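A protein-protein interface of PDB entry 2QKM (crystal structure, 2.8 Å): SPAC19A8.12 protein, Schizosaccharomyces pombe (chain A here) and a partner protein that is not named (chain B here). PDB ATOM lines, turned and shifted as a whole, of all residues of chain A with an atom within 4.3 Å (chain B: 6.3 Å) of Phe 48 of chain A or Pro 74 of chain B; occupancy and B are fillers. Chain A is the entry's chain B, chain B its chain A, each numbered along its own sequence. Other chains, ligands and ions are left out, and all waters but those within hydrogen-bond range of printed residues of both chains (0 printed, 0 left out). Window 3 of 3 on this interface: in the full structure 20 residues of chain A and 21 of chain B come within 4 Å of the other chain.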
ATOM      1  N   ARG A  18     -12.879  -7.998 -22.860  1.00  0.00           N
ATOM      2  CA  ARG A  18     -11.468  -7.623 -22.850  1.00  0.00           C
ATOM      3  C   ARG A  18     -11.196  -6.312 -23.567  1.00  0.00           C
ATOM      4  O   ARG A  18     -10.508  -5.462 -23.019  1.00  0.00           O
ATOM      5  CB  ARG A  18     -10.657  -8.721 -23.522  1.00  0.00           C
ATOM      6  CG  ARG A  18      -9.150  -8.737 -23.274  1.00  0.00           C
ATOM      7  CD  ARG A  18      -8.576 -10.063 -23.800  1.00  0.00           C
ATOM      8  NE  ARG A  18      -7.591 -10.573 -22.866  1.00  0.00           N
ATOM      9  CZ  ARG A  18      -7.815 -11.495 -21.934  1.00  0.00           C
ATOM     10  NH1 ARG A  18      -8.999 -12.073 -21.808  1.00  0.00           N
ATOM     11  NH2 ARG A  18      -6.829 -11.838 -21.124  1.00  0.00           N
ATOM     12  N   TRP A  43      -6.493  -9.498 -33.748  1.00  0.00           N
ATOM     13  CA  TRP A  43      -5.126  -9.979 -33.634  1.00  0.00           C
ATOM     14  C   TRP A  43      -4.933 -10.890 -32.394  1.00  0.00           C
ATOM     15  O   TRP A  43      -4.293 -11.942 -32.477  1.00  0.00           O
ATOM     16  CB  TRP A  43      -4.141  -8.803 -33.615  1.00  0.00           C
ATOM     17  CG  TRP A  43      -2.783  -9.159 -33.123  1.00  0.00           C
ATOM     18  CD1 TRP A  43      -1.800  -9.790 -33.821  1.00  0.00           C
ATOM     19  CD2 TRP A  43      -2.263  -8.948 -31.812  1.00  0.00           C
ATOM     20  NE1 TRP A  43      -0.690  -9.983 -33.034  1.00  0.00           N
ATOM     21  CE2 TRP A  43      -0.946  -9.476 -31.791  1.00  0.00           C
ATOM     22  CE3 TRP A  43      -2.779  -8.376 -30.642  1.00  0.00           C
ATOM     23  CZ2 TRP A  43      -0.134  -9.431 -30.643  1.00  0.00           C
ATOM     24  CZ3 TRP A  43      -1.978  -8.346 -29.503  1.00  0.00           C
ATOM     25  CH2 TRP A  43      -0.671  -8.861 -29.511  1.00  0.00           C
ATOM     26  N   PHE A  44      -5.465 -10.484 -31.250  1.00  0.00           N
ATOM     27  CA  PHE A  44      -5.384 -11.314 -30.049  1.00  0.00           C
ATOM     28  C   PHE A  44      -5.963 -12.706 -30.383  1.00  0.00           C
ATOM     29  O   PHE A  44      -5.424 -13.746 -29.979  1.00  0.00           O
ATOM     30  CB  PHE A  44      -6.192 -10.660 -28.930  1.00  0.00           C
ATOM     31  CG  PHE A  44      -5.921 -11.208 -27.555  1.00  0.00           C
ATOM     32  CD1 PHE A  44      -5.173 -10.476 -26.641  1.00  0.00           C
ATOM     33  CD2 PHE A  44      -6.470 -12.414 -27.144  1.00  0.00           C
ATOM     34  CE1 PHE A  44      -4.958 -10.935 -25.372  1.00  0.00           C
ATOM     35  CE2 PHE A  44      -6.248 -12.884 -25.864  1.00  0.00           C
ATOM     36  CZ  PHE A  44      -5.490 -12.144 -24.973  1.00  0.00           C
ATOM     37  N   TYR A  45      -7.058 -12.699 -31.142  1.00  0.00           N
ATOM     38  CA  TYR A  45      -7.742 -13.905 -31.533  1.00  0.00           C
ATOM     39  C   TYR A  45      -6.832 -14.782 -32.409  1.00  0.00           C
ATOM     40  O   TYR A  45      -6.499 -15.915 -32.038  1.00  0.00           O
ATOM     41  CB  TYR A  45      -9.033 -13.523 -32.269  1.00  0.00           C
ATOM     42  CG  TYR A  45      -9.837 -14.685 -32.805  1.00  0.00           C
ATOM     43  CD1 TYR A  45     -10.323 -15.690 -31.953  1.00  0.00           C
ATOM     44  CD2 TYR A  45     -10.132 -14.774 -34.160  1.00  0.00           C
ATOM     45  CE1 TYR A  45     -11.074 -16.744 -32.446  1.00  0.00           C
ATOM     46  CE2 TYR A  45     -10.877 -15.828 -34.660  1.00  0.00           C
ATOM     47  CZ  TYR A  45     -11.341 -16.808 -33.799  1.00  0.00           C
ATOM     48  OH  TYR A  45     -12.069 -17.852 -34.316  1.00  0.00           O
ATOM     49  N   GLU A  46      -6.425 -14.245 -33.557  1.00  0.00           N
ATOM     50  CA  GLU A  46      -5.628 -14.990 -34.507  1.00  0.00           C
ATOM     51  C   GLU A  46      -4.301 -15.438 -33.880  1.00  0.00           C
ATOM     52  O   GLU A  46      -3.842 -16.561 -34.102  1.00  0.00           O
ATOM     53  CB  GLU A  46      -5.369 -14.147 -35.760  1.00  0.00           C
ATOM     54  CG  GLU A  46      -6.593 -13.849 -36.652  1.00  0.00           C
ATOM     55  CD  GLU A  46      -7.167 -15.090 -37.383  1.00  0.00           C
ATOM     56  OE1 GLU A  46      -6.469 -16.139 -37.495  1.00  0.00           O
ATOM     57  OE2 GLU A  46      -8.335 -15.007 -37.845  1.00  0.00           O
ATOM     58  N   ASP A  47      -3.703 -14.567 -33.074  1.00  0.00           N
ATOM     59  CA  ASP A  47      -2.363 -14.810 -32.553  1.00  0.00           C
ATOM     60  C   ASP A  47      -2.284 -15.613 -31.276  1.00  0.00           C
ATOM     61  O   ASP A  47      -1.348 -16.377 -31.099  1.00  0.00           O
ATOM     62  CB  ASP A  47      -1.592 -13.504 -32.392  1.00  0.00           C
ATOM     63  CG  ASP A  47      -0.482 -13.377 -33.385  1.00  0.00           C
ATOM     64  OD1 ASP A  47      -0.599 -13.947 -34.491  1.00  0.00           O
ATOM     65  OD2 ASP A  47       0.524 -12.725 -33.054  1.00  0.00           O
ATOM     66  N   PHE A  48      -3.241 -15.447 -30.379  1.00  0.00           N
ATOM     67  CA  PHE A  48      -3.201 -16.184 -29.124  1.00  0.00           C
ATOM     68  C   PHE A  48      -4.289 -17.246 -28.977  1.00  0.00           C
ATOM     69  O   PHE A  48      -4.020 -18.358 -28.543  1.00  0.00           O
ATOM     70  CB  PHE A  48      -3.298 -15.226 -27.960  1.00  0.00           C
ATOM     71  CG  PHE A  48      -2.177 -14.218 -27.883  1.00  0.00           C
ATOM     72  CD1 PHE A  48      -0.861 -14.622 -27.651  1.00  0.00           C
ATOM     73  CD2 PHE A  48      -2.453 -12.852 -27.974  1.00  0.00           C
ATOM     74  CE1 PHE A  48       0.166 -13.692 -27.545  1.00  0.00           C
ATOM     75  CE2 PHE A  48      -1.426 -11.900 -27.860  1.00  0.00           C
ATOM     76  CZ  PHE A  48      -0.117 -12.326 -27.643  1.00  0.00           C
ATOM     77  N   ILE A  49      -5.529 -16.920 -29.307  1.00  0.00           N
ATOM     78  CA  ILE A  49      -6.607 -17.851 -29.027  1.00  0.00           C
ATOM     79  C   ILE A  49      -6.624 -19.018 -30.009  1.00  0.00           C
ATOM     80  O   ILE A  49      -6.479 -20.157 -29.596  1.00  0.00           O
ATOM     81  CB  ILE A  49      -7.973 -17.146 -28.888  1.00  0.00           C
ATOM     82  CG1 ILE A  49      -7.879 -16.044 -27.835  1.00  0.00           C
ATOM     83  CG2 ILE A  49      -9.056 -18.145 -28.516  1.00  0.00           C
ATOM     84  CD1 ILE A  49      -9.193 -15.386 -27.507  1.00  0.00           C
ATOM     85  N   ARG A  50      -6.787 -18.758 -31.302  1.00  0.00           N
ATOM     86  CA  ARG A  50      -6.762 -19.853 -32.300  1.00  0.00           C
ATOM     87  C   ARG A  50      -5.594 -20.840 -32.065  1.00  0.00           C
ATOM     88  O   ARG A  50      -5.721 -22.028 -32.327  1.00  0.00           O
ATOM     89  CB  ARG A  50      -6.708 -19.307 -33.726  1.00  0.00           C
ATOM     90  CG  ARG A  50      -7.988 -18.625 -34.177  1.00  0.00           C
ATOM     91  CD  ARG A  50      -8.007 -18.419 -35.686  1.00  0.00           C
ATOM     92  NE  ARG A  50      -8.380 -19.639 -36.411  1.00  0.00           N
ATOM     93  CZ  ARG A  50      -7.548 -20.439 -37.080  1.00  0.00           C
ATOM     94  NH1 ARG A  50      -6.254 -20.182 -37.149  1.00  0.00           N
ATOM     95  NH2 ARG A  50      -8.027 -21.507 -37.696  1.00  0.00           N
ATOM     96  N   ALA A  51      -4.480 -20.330 -31.543  1.00  0.00           N
ATOM     97  CA  ALA A  51      -3.321 -21.140 -31.193  1.00  0.00           C
ATOM     98  C   ALA A  51      -3.600 -22.282 -30.188  1.00  0.00           C
ATOM     99  O   ALA A  51      -2.951 -23.324 -30.236  1.00  0.00           O
ATOM    100  CB  ALA A  51      -2.202 -20.237 -30.678  1.00  0.00           C
ATOM    101  N   GLN A  52      -4.555 -22.087 -29.281  1.00  0.00           N
ATOM    102  CA  GLN A  52      -4.904 -23.131 -28.323  1.00  0.00           C
ATOM    103  C   GLN A  52      -6.202 -23.824 -28.658  1.00  0.00           C
ATOM    104  O   GLN A  52      -6.616 -24.751 -27.956  1.00  0.00           O
ATOM    105  CB  GLN A  52      -4.947 -22.615 -26.890  1.00  0.00           C
ATOM    106  CG  GLN A  52      -5.125 -21.136 -26.705  1.00  0.00           C
ATOM    107  CD  GLN A  52      -4.977 -20.751 -25.246  1.00  0.00           C
ATOM    108  OE1 GLN A  52      -5.949 -20.762 -24.489  1.00  0.00           O
ATOM    109  NE2 GLN A  52      -3.754 -20.421 -24.838  1.00  0.00           N
ATOM    110  N   ASN B  70      -5.720  -8.875 -19.381  1.00  0.00           N
ATOM    111  CA  ASN B  70      -4.605  -8.337 -20.147  1.00  0.00           C
ATOM    112  C   ASN B  70      -4.843  -8.231 -21.665  1.00  0.00           C
ATOM    113  O   ASN B  70      -5.318  -9.179 -22.291  1.00  0.00           O
ATOM    114  CB  ASN B  70      -3.386  -9.222 -19.841  1.00  0.00           C
ATOM    115  CG  ASN B  70      -2.106  -8.633 -20.321  1.00  0.00           C
ATOM    116  OD1 ASN B  70      -2.069  -7.513 -20.829  1.00  0.00           O
ATOM    117  ND2 ASN B  70      -1.035  -9.385 -20.178  1.00  0.00           N
ATOM    118  N   ARG B  71      -4.490  -7.078 -22.239  1.00  0.00           N
ATOM    119  CA  ARG B  71      -4.595  -6.798 -23.707  1.00  0.00           C
ATOM    120  C   ARG B  71      -3.399  -7.231 -24.566  1.00  0.00           C
ATOM    121  O   ARG B  71      -3.493  -7.234 -25.798  1.00  0.00           O
ATOM    122  CB  ARG B  71      -4.776  -5.298 -23.962  1.00  0.00           C
ATOM    123  CG  ARG B  71      -6.205  -4.779 -23.883  1.00  0.00           C
ATOM    124  CD  ARG B  71      -6.314  -3.328 -24.440  1.00  0.00           C
ATOM    125  NE  ARG B  71      -7.718  -2.952 -24.566  1.00  0.00           N
ATOM    126  CZ  ARG B  71      -8.513  -2.611 -23.545  1.00  0.00           C
ATOM    127  NH1 ARG B  71      -8.034  -2.577 -22.295  1.00  0.00           N
ATOM    128  NH2 ARG B  71      -9.800  -2.289 -23.781  1.00  0.00           N
ATOM    129  N   ASN B  72      -2.279  -7.555 -23.923  1.00  0.00           N
ATOM    130  CA  ASN B  72      -1.033  -7.814 -24.630  1.00  0.00           C
ATOM    131  C   ASN B  72      -0.745  -9.293 -24.825  1.00  0.00           C
ATOM    132  O   ASN B  72      -0.009  -9.675 -25.748  1.00  0.00           O
ATOM    133  CB  ASN B  72       0.132  -7.159 -23.893  1.00  0.00           C
ATOM    134  CG  ASN B  72       0.133  -5.651 -24.015  1.00  0.00           C
ATOM    135  OD1 ASN B  72      -0.084  -5.089 -25.101  1.00  0.00           O
ATOM    136  ND2 ASN B  72       0.399  -4.979 -22.898  1.00  0.00           N
ATOM    137  N   SER B  73      -1.310 -10.120 -23.942  1.00  0.00           N
ATOM    138  CA  SER B  73      -1.197 -11.581 -24.028  1.00  0.00           C
ATOM    139  C   SER B  73      -2.317 -12.171 -23.188  1.00  0.00           C
ATOM    140  O   SER B  73      -2.967 -11.434 -22.462  1.00  0.00           O
ATOM    141  CB  SER B  73       0.169 -12.057 -23.526  1.00  0.00           C
ATOM    142  OG  SER B  73       0.298 -11.900 -22.123  1.00  0.00           O
ATOM    143  N   PRO B  74      -2.570 -13.489 -23.303  1.00  0.00           N
ATOM    144  CA  PRO B  74      -3.571 -14.143 -22.456  1.00  0.00           C
ATOM    145  C   PRO B  74      -3.112 -14.357 -21.021  1.00  0.00           C
ATOM    146  O   PRO B  74      -3.711 -15.152 -20.307  1.00  0.00           O
ATOM    147  CB  PRO B  74      -3.767 -15.508 -23.129  1.00  0.00           C
ATOM    148  CG  PRO B  74      -3.097 -15.425 -24.444  1.00  0.00           C
ATOM    149  CD  PRO B  74      -1.993 -14.441 -24.267  1.00  0.00           C
ATOM    150  N   GLU B  75      -2.062 -13.662 -20.598  1.00  0.00           N
ATOM    151  CA  GLU B  75      -1.547 -13.833 -19.248  1.00  0.00           C
ATOM    152  C   GLU B  75      -2.074 -12.756 -18.314  1.00  0.00           C
ATOM    153  O   GLU B  75      -1.458 -11.706 -18.151  1.00  0.00           O
ATOM    154  CB  GLU B  75      -0.013 -13.844 -19.238  1.00  0.00           C
ATOM    155  CG  GLU B  75       0.602 -14.269 -17.896  1.00  0.00           C
ATOM    156  CD  GLU B  75       1.909 -13.551 -17.584  1.00  0.00           C
ATOM    157  OE1 GLU B  75       2.838 -14.206 -17.056  1.00  0.00           O
ATOM    158  OE2 GLU B  75       2.010 -12.332 -17.861  1.00  0.00           O
ATOM    159  N   ASN B  76      -3.206 -13.053 -17.684  1.00  0.00           N
ATOM    160  CA  ASN B  76      -3.894 -12.124 -16.796  1.00  0.00           C
ATOM    161  C   ASN B  76      -3.344 -12.097 -15.377  1.00  0.00           C
ATOM    162  O   ASN B  76      -2.655 -13.015 -14.952  1.00  0.00           O
ATOM    163  CB  ASN B  76      -5.371 -12.495 -16.739  1.00  0.00           C
ATOM    164  CG  ASN B  76      -5.988 -12.633 -18.107  1.00  0.00           C
ATOM    165  OD1 ASN B  76      -5.942 -11.711 -18.926  1.00  0.00           O
ATOM    166  ND2 ASN B  76      -6.578 -13.775 -18.364  1.00  0.00           N
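Of the 7 printed residues of chain B, 6 touch a printed residue of chain A.
Printed residues of chain B that touch a printed residue of chain A: Asn 70, Arg 71, Asn 72, Ser 73, Pro 74 and Asn 76.
Hydrophobic or aromatic side chains of chain B within 4 Å of the printed part of chain A: Pro 74.
Of the 11 printed residues of chain A, 4 touch a printed residue of chain B.
Along chain A the printed residues that touch a printed residue of chain B span positions 18 to 48.
Among the printed residues, no Asp or Glu carboxylate lies within 4 Å of a Lys or Arg side-chain nitrogen of the other chain.
OG of Ser 73 of chain B lies close to N of Glu 75 of chain B, 3.3 Å away.
O of Phe 44 of chain A lies within hydrogen-bond range of N of Ile 49 of chain A (3.2 Å).
The backbone NH (N) of Asn 72 of chain B is in hydrogen-bond range of the side-chain amide oxygen (OD1) of Asn 70 of chain B (3.1 Å).
The side-chain amide nitrogen (ND2) of Asn 70 of chain B sits at hydrogen-bond distance from the side-chain hydroxyl (OG) of Ser 73 of chain B, at 3.4 Å.
OD1 of Asn 76 of chain B lies within hydrogen-bond range of N of Asn 70 of chain B (2.9 Å).
The indole nitrogen (NE1) of Trp 43 of chain A sits at hydrogen-bond distance from the side-chain carboxylate (OD2) of Asp 47 of chain A (3.0 Å).
The side-chain amide nitrogen (ND2) of Asn 76 of chain B lies close to the guanidinium group (NH2) of Arg 18 of chain A (3.4 Å).
NE of Arg 18 of chain A lies within hydrogen-bond range of O of Asn 70 of chain B (2.7 Å).
NH2 of Arg 71 of chain B sits at hydrogen-bond distance from O of Arg 18 of chain A (3.3 Å).
O of Asn 72 of chain B touches CH2 of Trp 43 of chain A, 3.9 Å away.
CE1 of Phe 44 of chain A touches O of Asn 70 of chain B, at 3.6 Å.
Arg 71 of chain B touches Phe 44 of chain A (O to CD1, 3.7 Å).
Phe 44 of chain A touches Ser 73 of chain B (CE1 to O, 3.6 Å).
CZ of Phe 44 of chain A touches N of Pro 74 of chain B (3.6 Å).
CZ of Phe 48 of chain A touches O of Asn 72 of chain B (3.3 Å).
CZ of Phe 48 of chain A touches CA of Ser 73 of chain B, at 3.8 Å.
Pro 74 of chain B touches Phe 48 of chain A (CG to CB, 3.5 Å).
Printed residues of chain B within 4 Å of Arg 18 of chain A: Asn 70, Arg 71 and Asn 76.
Printed residues of chain B within 4 Å of Phe 44 of chain A: Asn 70 (3.6 Å), Arg 71 (3.7 Å), Ser 73 (3.6 Å) and Pro 74 (3.6 Å).
Phe 48 of chain A touches just these residues of chain B: Asn 72, Ser 73 and Pro 74.
Printed residues of chain A within 4 Å of Asn 70 of chain B: Arg 18 (2.7 Å) and Phe 44 (3.6 Å).
Of the printed residues of chain A, Ser 73 of chain B touches Phe 44 (3.6 Å) and Phe 48 (3.8 Å).
Of chain A, only Phe 44 and Phe 48 come within 4 Å of Pro 74 of chain B.
Printed residues of chain A within 4 Å of Asn 76 of chain B: Arg 18 (2.4 Å).
The nearest printed residue of chain B that does not touch Phe 44 of chain A is Asn 72 of chain B (4.5 Å).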
